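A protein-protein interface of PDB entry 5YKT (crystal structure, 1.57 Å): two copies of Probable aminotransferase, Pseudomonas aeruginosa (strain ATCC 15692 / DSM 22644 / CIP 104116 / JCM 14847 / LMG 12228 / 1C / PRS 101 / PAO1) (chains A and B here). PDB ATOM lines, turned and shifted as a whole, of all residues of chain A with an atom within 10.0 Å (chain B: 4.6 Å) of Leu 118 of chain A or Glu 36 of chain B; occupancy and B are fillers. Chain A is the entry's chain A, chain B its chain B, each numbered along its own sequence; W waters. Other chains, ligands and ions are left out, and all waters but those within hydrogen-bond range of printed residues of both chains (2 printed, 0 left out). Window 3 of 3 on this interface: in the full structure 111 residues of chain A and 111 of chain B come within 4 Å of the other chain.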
ATOM      1  N   LEU A 112       6.757 -22.615   8.152  1.00  0.00           N
ATOM      2  CA  LEU A 112       5.950 -22.962   6.997  1.00  0.00           C
ATOM      3  C   LEU A 112       6.833 -23.052   5.768  1.00  0.00           C
ATOM      4  O   LEU A 112       7.905 -22.435   5.716  1.00  0.00           O
ATOM      5  CB  LEU A 112       4.877 -21.915   6.724  1.00  0.00           C
ATOM      6  CG  LEU A 112       3.747 -21.854   7.758  1.00  0.00           C
ATOM      7  CD1 LEU A 112       2.940 -20.568   7.611  1.00  0.00           C
ATOM      8  CD2 LEU A 112       2.863 -23.070   7.627  1.00  0.00           C
ATOM      9  N   PRO A 113       6.372 -23.822   4.780  1.00  0.00           N
ATOM     10  CA  PRO A 113       7.097 -23.899   3.519  1.00  0.00           C
ATOM     11  C   PRO A 113       6.845 -22.700   2.624  1.00  0.00           C
ATOM     12  O   PRO A 113       5.860 -21.984   2.783  1.00  0.00           O
ATOM     13  CB  PRO A 113       6.526 -25.156   2.880  1.00  0.00           C
ATOM     14  CG  PRO A 113       5.129 -25.255   3.407  1.00  0.00           C
ATOM     15  CD  PRO A 113       5.233 -24.748   4.813  1.00  0.00           C
ATOM     16  N   THR A 114       7.737 -22.521   1.657  1.00  0.00           N
ATOM     17  CA  THR A 114       7.562 -21.574   0.560  1.00  0.00           C
ATOM     18  C   THR A 114       7.694 -22.324  -0.764  1.00  0.00           C
ATOM     19  O   THR A 114       7.987 -23.513  -0.788  1.00  0.00           O
ATOM     20  CB  THR A 114       8.644 -20.484   0.591  1.00  0.00           C
ATOM     21  OG1 THR A 114       9.929 -21.086   0.361  1.00  0.00           O
ATOM     22  CG2 THR A 114       8.686 -19.752   1.934  1.00  0.00           C
ATOM     23  N   GLU A 115       7.532 -21.609  -1.877  1.00  0.00           N
ATOM     24  CA  GLU A 115       7.662 -22.257  -3.194  1.00  0.00           C
ATOM     25  C   GLU A 115       9.042 -22.845  -3.429  1.00  0.00           C
ATOM     26  O   GLU A 115       9.166 -23.811  -4.171  1.00  0.00           O
ATOM     27  CB  GLU A 115       7.287 -21.294  -4.330  1.00  0.00           C
ATOM     28  CG  GLU A 115       5.804 -21.006  -4.372  1.00  0.00           C
ATOM     29  CD  GLU A 115       5.387 -20.114  -5.525  1.00  0.00           C
ATOM     30  OE1 GLU A 115       6.194 -19.249  -5.937  1.00  0.00           O
ATOM     31  OE2 GLU A 115       4.242 -20.285  -6.017  1.00  0.00           O
ATOM     32  N   ASP A 116      10.070 -22.306  -2.776  1.00  0.00           N
ATOM     33  CA  ASP A 116      11.401 -22.922  -2.888  1.00  0.00           C
ATOM     34  C   ASP A 116      11.450 -24.366  -2.377  1.00  0.00           C
ATOM     35  O   ASP A 116      12.244 -25.157  -2.889  1.00  0.00           O
ATOM     36  CB  ASP A 116      12.450 -22.093  -2.171  1.00  0.00           C
ATOM     37  CG  ASP A 116      12.653 -20.734  -2.819  1.00  0.00           C
ATOM     38  OD1 ASP A 116      12.397 -20.568  -4.040  1.00  0.00           O
ATOM     39  OD2 ASP A 116      13.092 -19.798  -2.122  1.00  0.00           O
ATOM     40  N   SER A 117      10.614 -24.748  -1.409  1.00  0.00           N
ATOM     41  CA  SER A 117      10.577 -26.131  -0.956  1.00  0.00           C
ATOM     42  C   SER A 117      10.156 -27.085  -2.069  1.00  0.00           C
ATOM     43  O   SER A 117      10.649 -28.203  -2.132  1.00  0.00           O
ATOM     44  CB  SER A 117       9.668 -26.315   0.268  1.00  0.00           C
ATOM     45  OG  SER A 117       8.322 -26.082  -0.067  1.00  0.00           O
ATOM     46  N   LEU A 118       9.249 -26.646  -2.946  1.00  0.00           N
ATOM     47  CA  LEU A 118       8.837 -27.473  -4.067  1.00  0.00           C
ATOM     48  C   LEU A 118      10.014 -27.752  -4.987  1.00  0.00           C
ATOM     49  O   LEU A 118      10.256 -28.907  -5.342  1.00  0.00           O
ATOM     50  CB  LEU A 118       7.722 -26.770  -4.860  1.00  0.00           C
ATOM     51  CG  LEU A 118       6.380 -26.685  -4.154  1.00  0.00           C
ATOM     52  CD1 LEU A 118       5.538 -25.603  -4.820  1.00  0.00           C
ATOM     53  CD2 LEU A 118       5.714 -28.042  -4.248  1.00  0.00           C
ATOM     54  N   TRP A 119      10.731 -26.697  -5.362  1.00  0.00           N
ATOM     55  CA  TRP A 119      11.827 -26.833  -6.298  1.00  0.00           C
ATOM     56  C   TRP A 119      12.953 -27.671  -5.676  1.00  0.00           C
ATOM     57  O   TRP A 119      13.510 -28.580  -6.312  1.00  0.00           O
ATOM     58  CB  TRP A 119      12.347 -25.448  -6.686  1.00  0.00           C
ATOM     59  CG  TRP A 119      13.297 -25.489  -7.828  1.00  0.00           C
ATOM     60  CD1 TRP A 119      13.001 -25.286  -9.144  1.00  0.00           C
ATOM     61  CD2 TRP A 119      14.702 -25.773  -7.776  1.00  0.00           C
ATOM     62  NE1 TRP A 119      14.140 -25.369  -9.908  1.00  0.00           N
ATOM     63  CE2 TRP A 119      15.195 -25.688  -9.096  1.00  0.00           C
ATOM     64  CE3 TRP A 119      15.603 -26.052  -6.741  1.00  0.00           C
ATOM     65  CZ2 TRP A 119      16.534 -25.921  -9.405  1.00  0.00           C
ATOM     66  CZ3 TRP A 119      16.923 -26.288  -7.055  1.00  0.00           C
ATOM     67  CH2 TRP A 119      17.382 -26.215  -8.366  1.00  0.00           C
ATOM     68  N   VAL A 120      13.324 -27.361  -4.441  1.00  0.00           N
ATOM     69  CA  VAL A 120      14.449 -28.048  -3.799  1.00  0.00           C
ATOM     70  C   VAL A 120      14.179 -29.515  -3.547  1.00  0.00           C
ATOM     71  O   VAL A 120      15.030 -30.347  -3.776  1.00  0.00           O
ATOM     72  CB  VAL A 120      14.879 -27.340  -2.506  1.00  0.00           C
ATOM     73  CG1 VAL A 120      15.888 -28.163  -1.718  1.00  0.00           C
ATOM     74  CG2 VAL A 120      15.471 -25.960  -2.817  1.00  0.00           C
ATOM     75  N   GLY A 121      12.991 -29.866  -3.096  1.00  0.00           N
ATOM     76  CA  GLY A 121      12.686 -31.278  -2.898  1.00  0.00           C
ATOM     77  C   GLY A 121      12.861 -32.103  -4.161  1.00  0.00           C
ATOM     78  O   GLY A 121      13.467 -33.189  -4.140  1.00  0.00           O
ATOM     79  N   ALA A 122      12.346 -31.591  -5.276  1.00  0.00           N
ATOM     80  CA  ALA A 122      12.448 -32.267  -6.551  1.00  0.00           C
ATOM     81  C   ALA A 122      13.898 -32.347  -7.025  1.00  0.00           C
ATOM     82  O   ALA A 122      14.313 -33.367  -7.561  1.00  0.00           O
ATOM     83  CB  ALA A 122      11.611 -31.560  -7.595  1.00  0.00           C
ATOM     84  N   GLU A 123      14.646 -31.271  -6.793  1.00  0.00           N
ATOM     85  CA  GLU A 123      16.061 -31.220  -7.150  1.00  0.00           C
ATOM     86  C   GLU A 123      16.890 -32.223  -6.360  1.00  0.00           C
ATOM     87  O   GLU A 123      17.765 -32.882  -6.937  1.00  0.00           O
ATOM     88  CB  GLU A 123      16.621 -29.807  -6.971  1.00  0.00           C
ATOM     89  CG  GLU A 123      18.139 -29.679  -7.093  1.00  0.00           C
ATOM     90  CD  GLU A 123      18.702 -29.989  -8.463  1.00  0.00           C
ATOM     91  OE1 GLU A 123      17.951 -30.124  -9.470  1.00  0.00           O
ATOM     92  OE2 GLU A 123      19.956 -30.081  -8.542  1.00  0.00           O
ATOM     93  N   LEU A 124      16.643 -32.349  -5.064  1.00  0.00           N
ATOM     94  CA  LEU A 124      17.366 -33.328  -4.240  1.00  0.00           C
ATOM     95  C   LEU A 124      17.148 -34.736  -4.742  1.00  0.00           C
ATOM     96  O   LEU A 124      18.103 -35.530  -4.856  1.00  0.00           O
ATOM     97  CB  LEU A 124      16.941 -33.223  -2.790  1.00  0.00           C
ATOM     98  CG  LEU A 124      17.389 -31.959  -2.056  1.00  0.00           C
ATOM     99  CD1 LEU A 124      16.669 -31.782  -0.741  1.00  0.00           C
ATOM    100  CD2 LEU A 124      18.892 -31.991  -1.818  1.00  0.00           C
ATOM    101  N   ALA A 125      15.888 -35.071  -5.043  1.00  0.00           N
ATOM    102  CA  ALA A 125      15.571 -36.397  -5.568  1.00  0.00           C
ATOM    103  C   ALA A 125      16.234 -36.662  -6.913  1.00  0.00           C
ATOM    104  O   ALA A 125      16.736 -37.756  -7.148  1.00  0.00           O
ATOM    105  CB  ALA A 125      14.059 -36.570  -5.659  1.00  0.00           C
ATOM    106  N   ARG A 126      16.232 -35.654  -7.783  1.00  0.00           N
ATOM    107  CA  ARG A 126      16.874 -35.758  -9.089  1.00  0.00           C
ATOM    108  C   ARG A 126      18.383 -35.943  -8.960  1.00  0.00           C
ATOM    109  O   ARG A 126      18.965 -36.849  -9.564  1.00  0.00           O
ATOM    110  CB  ARG A 126      16.595 -34.510  -9.924  1.00  0.00           C
ATOM    111  CG  ARG A 126      17.174 -34.550 -11.341  1.00  0.00           C
ATOM    112  CD  ARG A 126      17.440 -33.160 -11.899  1.00  0.00           C
ATOM    113  NE  ARG A 126      18.510 -32.450 -11.179  1.00  0.00           N
ATOM    114  CZ  ARG A 126      19.819 -32.691 -11.311  1.00  0.00           C
ATOM    115  NH1 ARG A 126      20.286 -33.657 -12.107  1.00  0.00           N
ATOM    116  NH2 ARG A 126      20.675 -31.979 -10.611  1.00  0.00           N
ATOM    117  N   PRO A 131      14.336 -40.702  -2.968  1.00  0.00           N
ATOM    118  CA  PRO A 131      13.090 -39.946  -3.184  1.00  0.00           C
ATOM    119  C   PRO A 131      12.661 -38.971  -2.097  1.00  0.00           C
ATOM    120  O   PRO A 131      12.020 -37.984  -2.439  1.00  0.00           O
ATOM    121  CB  PRO A 131      12.025 -41.047  -3.315  1.00  0.00           C
ATOM    122  CG  PRO A 131      12.622 -42.249  -2.672  1.00  0.00           C
ATOM    123  CD  PRO A 131      14.100 -42.159  -2.875  1.00  0.00           C
ATOM    124  N   TYR A 132      13.003 -39.216  -0.837  1.00  0.00           N
ATOM    125  CA  TYR A 132      12.403 -38.447   0.276  1.00  0.00           C
ATOM    126  C   TYR A 132      13.449 -37.754   1.126  1.00  0.00           C
ATOM    127  O   TYR A 132      14.429 -38.371   1.488  1.00  0.00           O
ATOM    128  CB  TYR A 132      11.552 -39.354   1.191  1.00  0.00           C
ATOM    129  CG  TYR A 132      10.411 -39.980   0.465  1.00  0.00           C
ATOM    130  CD1 TYR A 132       9.283 -39.240   0.137  1.00  0.00           C
ATOM    131  CD2 TYR A 132      10.469 -41.310   0.067  1.00  0.00           C
ATOM    132  CE1 TYR A 132       8.236 -39.822  -0.563  1.00  0.00           C
ATOM    133  CE2 TYR A 132       9.433 -41.889  -0.632  1.00  0.00           C
ATOM    134  CZ  TYR A 132       8.320 -41.145  -0.929  1.00  0.00           C
ATOM    135  OH  TYR A 132       7.291 -41.735  -1.643  1.00  0.00           O
ATOM    136  N   TRP A 133      13.187 -36.503   1.477  1.00  0.00           N
ATOM    137  CA  TRP A 133      14.168 -35.613   2.116  1.00  0.00           C
ATOM    138  C   TRP A 133      13.592 -34.915   3.342  1.00  0.00           C
ATOM    139  O   TRP A 133      12.355 -34.797   3.498  1.00  0.00           O
ATOM    140  CB  TRP A 133      14.693 -34.597   1.085  1.00  0.00           C
ATOM    141  CG  TRP A 133      15.379 -35.319  -0.017  1.00  0.00           C
ATOM    142  CD1 TRP A 133      14.797 -35.905  -1.084  1.00  0.00           C
ATOM    143  CD2 TRP A 133      16.764 -35.663  -0.079  1.00  0.00           C
ATOM    144  NE1 TRP A 133      15.729 -36.589  -1.838  1.00  0.00           N
ATOM    145  CE2 TRP A 133      16.948 -36.450  -1.242  1.00  0.00           C
ATOM    146  CE3 TRP A 133      17.886 -35.336   0.698  1.00  0.00           C
ATOM    147  CZ2 TRP A 133      18.190 -36.928  -1.619  1.00  0.00           C
ATOM    148  CZ3 TRP A 133      19.108 -35.827   0.328  1.00  0.00           C
ATOM    149  CH2 TRP A 133      19.255 -36.613  -0.819  1.00  0.00           C
ATOM    150  N   VAL A 135      15.121 -31.446   6.080  1.00  0.00           N
ATOM    151  CA  VAL A 135      16.149 -30.441   6.312  1.00  0.00           C
ATOM    152  C   VAL A 135      16.408 -30.296   7.805  1.00  0.00           C
ATOM    153  O   VAL A 135      15.469 -30.328   8.609  1.00  0.00           O
ATOM    154  CB  VAL A 135      15.718 -29.078   5.738  1.00  0.00           C
ATOM    155  CG1 VAL A 135      16.796 -28.025   5.932  1.00  0.00           C
ATOM    156  CG2 VAL A 135      15.382 -29.199   4.270  1.00  0.00           C
ATOM    157  N   GLY A 331      14.598 -26.275   8.142  1.00  0.00           N
ATOM    158  CA  GLY A 331      13.741 -26.216   6.962  1.00  0.00           C
ATOM    159  C   GLY A 331      13.105 -24.875   6.729  1.00  0.00           C
ATOM    160  O   GLY A 331      12.032 -24.791   6.155  1.00  0.00           O
ATOM    161  N   LEU A 336      16.062 -22.689   2.424  1.00  0.00           N
ATOM    162  CA  LEU A 336      15.580 -23.245   1.161  1.00  0.00           C
ATOM    163  C   LEU A 336      15.895 -22.306  -0.012  1.00  0.00           C
ATOM    164  O   LEU A 336      16.232 -22.777  -1.098  1.00  0.00           O
ATOM    165  CB  LEU A 336      14.084 -23.573   1.219  1.00  0.00           C
ATOM    166  CG  LEU A 336      13.705 -24.966   1.763  1.00  0.00           C
ATOM    167  CD1 LEU A 336      14.122 -26.042   0.789  1.00  0.00           C
ATOM    168  CD2 LEU A 336      14.297 -25.288   3.130  1.00  0.00           C
ATOM    169  N   ALA A 337      15.822 -20.991   0.207  1.00  0.00           N
ATOM    170  CA  ALA A 337      16.202 -20.032  -0.820  1.00  0.00           C
ATOM    171  C   ALA A 337      17.671 -20.185  -1.201  1.00  0.00           C
ATOM    172  O   ALA A 337      18.005 -20.182  -2.378  1.00  0.00           O
ATOM    173  CB  ALA A 337      15.935 -18.606  -0.370  1.00  0.00           C
ATOM    174  N   ARG A 340      18.232 -23.490  -3.134  1.00  0.00           N
ATOM    175  CA  ARG A 340      17.786 -23.397  -4.518  1.00  0.00           C
ATOM    176  C   ARG A 340      18.848 -22.708  -5.379  1.00  0.00           C
ATOM    177  O   ARG A 340      19.220 -23.197  -6.448  1.00  0.00           O
ATOM    178  CB  ARG A 340      16.453 -22.672  -4.594  1.00  0.00           C
ATOM    179  CG  ARG A 340      15.964 -22.482  -6.000  1.00  0.00           C
ATOM    180  CD  ARG A 340      14.546 -22.006  -6.004  1.00  0.00           C
ATOM    181  NE  ARG A 340      14.017 -21.952  -7.358  1.00  0.00           N
ATOM    182  CZ  ARG A 340      12.728 -21.784  -7.643  1.00  0.00           C
ATOM    183  NH1 ARG A 340      11.827 -21.613  -6.673  1.00  0.00           N
ATOM    184  NH2 ARG A 340      12.340 -21.792  -8.909  1.00  0.00           N
ATOM    185  N   PHE A 343      22.024 -25.116  -5.731  1.00  0.00           N
ATOM    186  CA  PHE A 343      21.835 -26.224  -6.657  1.00  0.00           C
ATOM    187  C   PHE A 343      21.640 -25.757  -8.109  1.00  0.00           C
ATOM    188  O   PHE A 343      22.124 -26.398  -9.038  1.00  0.00           O
ATOM    189  CB  PHE A 343      20.658 -27.108  -6.224  1.00  0.00           C
ATOM    190  CG  PHE A 343      20.904 -27.899  -4.949  1.00  0.00           C
ATOM    191  CD1 PHE A 343      22.057 -28.639  -4.749  1.00  0.00           C
ATOM    192  CD2 PHE A 343      19.969 -27.877  -3.934  1.00  0.00           C
ATOM    193  CE1 PHE A 343      22.256 -29.353  -3.593  1.00  0.00           C
ATOM    194  CE2 PHE A 343      20.151 -28.595  -2.779  1.00  0.00           C
ATOM    195  CZ  PHE A 343      21.308 -29.330  -2.599  1.00  0.00           C
ATOM    196  N   GLN B  32      -2.569 -28.106  -3.428  1.00  0.00           N
ATOM    197  CA  GLN B  32      -1.883 -28.603  -4.626  1.00  0.00           C
ATOM    198  C   GLN B  32      -0.390 -28.682  -4.361  1.00  0.00           C
ATOM    199  O   GLN B  32       0.245 -29.686  -4.706  1.00  0.00           O
ATOM    200  CB  GLN B  32      -2.187 -27.704  -5.824  1.00  0.00           C
ATOM    201  CG  GLN B  32      -1.562 -28.129  -7.148  1.00  0.00           C
ATOM    202  CD  GLN B  32      -1.678 -27.056  -8.230  1.00  0.00           C
ATOM    203  OE1 GLN B  32      -2.359 -26.038  -8.058  1.00  0.00           O
ATOM    204  NE2 GLN B  32      -1.002 -27.281  -9.352  1.00  0.00           N
ATOM    205  N   ALA B  33       0.173 -27.636  -3.761  1.00  0.00           N
ATOM    206  CA  ALA B  33       1.592 -27.646  -3.411  1.00  0.00           C
ATOM    207  C   ALA B  33       1.945 -28.804  -2.469  1.00  0.00           C
ATOM    208  O   ALA B  33       2.973 -29.449  -2.625  1.00  0.00           O
ATOM    209  CB  ALA B  33       2.017 -26.322  -2.813  1.00  0.00           C
ATOM    210  N   TYR B  34       1.051 -29.092  -1.521  1.00  0.00           N
ATOM    211  CA  TYR B  34       1.284 -30.191  -0.585  1.00  0.00           C
ATOM    212  C   TYR B  34       1.329 -31.558  -1.290  1.00  0.00           C
ATOM    213  O   TYR B  34       2.160 -32.424  -0.957  1.00  0.00           O
ATOM    214  CB  TYR B  34       0.204 -30.202   0.499  1.00  0.00           C
ATOM    215  CG  TYR B  34       0.433 -31.223   1.605  1.00  0.00           C
ATOM    216  CD1 TYR B  34       1.539 -31.152   2.432  1.00  0.00           C
ATOM    217  CD2 TYR B  34      -0.483 -32.241   1.823  1.00  0.00           C
ATOM    218  CE1 TYR B  34       1.732 -32.065   3.449  1.00  0.00           C
ATOM    219  CE2 TYR B  34      -0.290 -33.171   2.830  1.00  0.00           C
ATOM    220  CZ  TYR B  34       0.790 -33.071   3.647  1.00  0.00           C
ATOM    221  OH  TYR B  34       0.936 -34.029   4.642  1.00  0.00           O
ATOM    222  N   ARG B  35       0.439 -31.765  -2.261  1.00  0.00           N
ATOM    223  CA  ARG B  35       0.441 -32.984  -3.075  1.00  0.00           C
ATOM    224  C   ARG B  35       1.800 -33.175  -3.741  1.00  0.00           C
ATOM    225  O   ARG B  35       2.347 -34.297  -3.750  1.00  0.00           O
ATOM    226  CB  ARG B  35      -0.681 -32.977  -4.121  1.00  0.00           C
ATOM    227  CG  ARG B  35      -2.070 -33.075  -3.490  1.00  0.00           C
ATOM    228  CD  ARG B  35      -3.179 -33.329  -4.487  1.00  0.00           C
ATOM    229  NE  ARG B  35      -3.279 -32.303  -5.520  1.00  0.00           N
ATOM    230  CZ  ARG B  35      -4.081 -31.228  -5.507  1.00  0.00           C
ATOM    231  NH1 ARG B  35      -4.884 -30.947  -4.471  1.00  0.00           N
ATOM    232  NH2 ARG B  35      -4.047 -30.386  -6.551  1.00  0.00           N
ATOM    233  N   GLU B  36       2.367 -32.089  -4.272  1.00  0.00           N
ATOM    234  CA  GLU B  36       3.688 -32.183  -4.894  1.00  0.00           C
ATOM    235  C   GLU B  36       4.786 -32.379  -3.858  1.00  0.00           C
ATOM    236  O   GLU B  36       5.686 -33.208  -4.048  1.00  0.00           O
ATOM    237  CB  GLU B  36       3.966 -30.934  -5.726  1.00  0.00           C
ATOM    238  CG  GLU B  36       5.315 -30.937  -6.459  1.00  0.00           C
ATOM    239  CD  GLU B  36       5.456 -32.000  -7.545  1.00  0.00           C
ATOM    240  OE1 GLU B  36       4.437 -32.593  -7.980  1.00  0.00           O
ATOM    241  OE2 GLU B  36       6.613 -32.227  -7.972  1.00  0.00           O
ATOM    242  N   ASN B  37       4.717 -31.640  -2.756  1.00  0.00           N
ATOM    243  CA  ASN B  37       5.759 -31.729  -1.737  1.00  0.00           C
ATOM    244  C   ASN B  37       5.790 -33.088  -1.047  1.00  0.00           C
ATOM    245  O   ASN B  37       6.855 -33.522  -0.619  1.00  0.00           O
ATOM    246  CB  ASN B  37       5.648 -30.594  -0.706  1.00  0.00           C
ATOM    247  CG  ASN B  37       6.561 -29.407  -1.007  1.00  0.00           C
ATOM    248  OD1 ASN B  37       7.521 -29.507  -1.774  1.00  0.00           O
ATOM    249  ND2 ASN B  37       6.275 -28.286  -0.358  1.00  0.00           N
ATOM    250  N   ARG B  38       4.644 -33.767  -0.949  1.00  0.00           N
ATOM    251  CA  ARG B  38       4.641 -35.114  -0.386  1.00  0.00           C
ATOM    252  C   ARG B  38       5.424 -36.126  -1.233  1.00  0.00           C
ATOM    253  O   ARG B  38       5.805 -37.178  -0.735  1.00  0.00           O
ATOM    254  CB  ARG B  38       3.203 -35.629  -0.131  1.00  0.00           C
ATOM    255  CG  ARG B  38       2.550 -35.052   1.104  1.00  0.00           C
ATOM    256  CD  ARG B  38       3.082 -35.627   2.417  1.00  0.00           C
ATOM    257  NE  ARG B  38       2.805 -37.037   2.551  1.00  0.00           N
ATOM    258  CZ  ARG B  38       1.667 -37.560   3.011  1.00  0.00           C
ATOM    259  NH1 ARG B  38       0.684 -36.790   3.503  1.00  0.00           N
ATOM    260  NH2 ARG B  38       1.542 -38.878   3.024  1.00  0.00           N
ATOM    261  N   ARG B  39       5.664 -35.814  -2.505  1.00  0.00           N
ATOM    262  CA  ARG B  39       6.455 -36.698  -3.369  1.00  0.00           C
ATOM    263  C   ARG B  39       7.931 -36.723  -3.013  1.00  0.00           C
ATOM    264  O   ARG B  39       8.592 -37.721  -3.293  1.00  0.00           O
ATOM    265  CB  ARG B  39       6.316 -36.296  -4.845  1.00  0.00           C
ATOM    266  CG  ARG B  39       4.874 -36.373  -5.359  1.00  0.00           C
ATOM    267  CD  ARG B  39       4.797 -35.849  -6.781  1.00  0.00           C
ATOM    268  NE  ARG B  39       5.473 -36.789  -7.671  1.00  0.00           N
ATOM    269  CZ  ARG B  39       5.959 -36.507  -8.882  1.00  0.00           C
ATOM    270  NH1 ARG B  39       5.886 -35.279  -9.402  1.00  0.00           N
ATOM    271  NH2 ARG B  39       6.534 -37.475  -9.586  1.00  0.00           N
ATOM    272  N   HIS B  40       8.438 -35.628  -2.466  1.00  0.00           N
ATOM    273  CA  HIS B  40       9.874 -35.465  -2.223  1.00  0.00           C
ATOM    274  C   HIS B  40      10.294 -35.165  -0.792  1.00  0.00           C
ATOM    275  O   HIS B  40      11.466 -35.302  -0.481  1.00  0.00           O
ATOM    276  CB  HIS B  40      10.488 -34.385  -3.145  1.00  0.00           C
ATOM    277  CG  HIS B  40       9.922 -34.326  -4.526  1.00  0.00           C
ATOM    278  ND1 HIS B  40      10.185 -35.282  -5.477  1.00  0.00           N
ATOM    279  CD2 HIS B  40       9.158 -33.386  -5.134  1.00  0.00           C
ATOM    280  CE1 HIS B  40       9.583 -34.959  -6.608  1.00  0.00           C
ATOM    281  NE2 HIS B  40       8.943 -33.818  -6.425  1.00  0.00           N
ATOM    282  N   LEU B  60       1.519 -22.625   2.098  1.00  0.00           N
ATOM    283  CA  LEU B  60       2.738 -22.136   1.435  1.00  0.00           C
ATOM    284  C   LEU B  60       2.738 -20.620   1.451  1.00  0.00           C
ATOM    285  O   LEU B  60       1.803 -19.997   0.946  1.00  0.00           O
ATOM    286  CB  LEU B  60       2.906 -22.662   0.001  1.00  0.00           C
ATOM    287  CG  LEU B  60       3.938 -23.812  -0.074  1.00  0.00           C
ATOM    288  CD1 LEU B  60       3.223 -25.058   0.416  1.00  0.00           C
ATOM    289  CD2 LEU B  60       4.488 -24.015  -1.465  1.00  0.00           C
HETATM  290  O   HOH W   1       7.983 -40.008  -4.507  1.00  0.00           O
HETATM  291  O   HOH W   2      11.001 -37.919  -4.984  1.00  0.00           O
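The side-chain hydroxyl of Ser 117 of chain A sits at hydrogen-bond distance from the backbone carbonyl oxygen of Thr 114 of chain A (2.7 Å).
OE1 of Glu 36 of chain B lies within salt-bridge range of NH1 of Arg 39 of chain B (3.4 Å).
NH1 of Arg 38 of chain B sits at hydrogen-bond distance from OH of Tyr 34 of chain B (3.0 Å).
OE2 of Glu 36 of chain B is in hydrogen-bond range of NE2 of His 40 of chain B, at 3.2 Å.
OG1 of Thr 114 of chain A sits close to N of Asp 116 of chain A, at 3.4 Å.
Water W1 lies within hydrogen-bond range of the backbone carbonyl oxygen (O) of Arg 39 of chain B (2.7 Å) and the side-chain hydroxyl (OH) of Tyr 132 of chain A (3.4 Å).
Water W2 lies within hydrogen-bond range of the backbone carbonyl oxygen (O) of Pro 131 of chain A (2.7 Å), a ring nitrogen (ND1) of His 40 of chain B (2.8 Å) and the backbone carbonyl oxygen (O) of Arg 39 of chain B (2.9 Å).
The backbone carbonyl oxygen of Pro 131 of chain A sits close to the backbone carbonyl oxygen of His 40 of chain B (3.4 Å).
N of Trp 133 of chain A lies within hydrogen-bond range of O of His 40 of chain B (2.9 Å).
The side-chain hydroxyl (OG) of Ser 117 of chain A lies within hydrogen-bond range of the side-chain amide nitrogen (ND2) of Asn 37 of chain B (3.0 Å).
Printed residues of chain A that touch a printed residue of chain B: Pro 113, Thr 114, Glu 115, Ser 117, Leu 118, Gly 121, Ala 122, Pro 131, Tyr 132 and Trp 133.
Hydrophobic or aromatic side chains of chain A within 4 Å of the printed part of chain B: Pro 113, Leu 118, Ala 122, Tyr 132 and Trp 133.
Among the printed residues, 16 pairs touch across the chains.
Of chain B, only Ala 33, Glu 36, Asn 37 and Leu 60 come within 4 Å of Leu 118 of chain A.
Of the printed residues of chain A, Glu 36 of chain B touches Leu 118.
Asn 37 of chain B touches just these residues of chain A: Ser 117 and Leu 118.
Of the printed residues of chain A, Arg 39 of chain B touches Pro 131 and Tyr 132.
Printed residues of chain B within 4 Å of Ala 122 of chain A: His 40 (3.7 Å).
Printed residues of chain A within 4 Å of Arg 38 of chain B: Tyr 132 (3.6 Å).
Printed residues of chain B within 4 Å of Gly 121 of chain A: His 40 (3.4 Å).
The nearest printed residue of chain B that does not touch Leu 118 of chain A is His 40 of chain B (4.6 Å).
The nearest printed residue of chain A that does not touch Leu 60 of chain B is Ser 117 of chain A (4.6 Å).
Among the printed residues, merely in contact across the chains: Leu 118 of chain A with Asn 37 of chain B (3.3 Å), Gly 121 of chain A with His 40 of chain B (3.4 Å), Tyr 132 of chain A with His 40 of chain B (3.4 Å), Pro 113 of chain A with Leu 60 of chain B (3.4 Å), Tyr 132 of chain A with Arg 39 of chain B (3.5 Å), Leu 118 of chain A with Ala 33 of chain B (3.5 Å), Pro 131 of chain A with Arg 39 of chain B (3.5 Å), Tyr 132 of chain A with Arg 38 of chain B (3.6 Å), Thr 114 of chain A with Leu 60 of chain B (3.6 Å), Ala 122 of chain A with His 40 of chain B (3.7 Å), Leu 118 of chain A with Glu 36 of chain B (3.7 Å), Leu 118 of chain A with Leu 60 of chain B (3.9 Å) and Glu 115 of chain A with Leu 60 of chain B (3.9 Å).
No position is printed for both chains.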
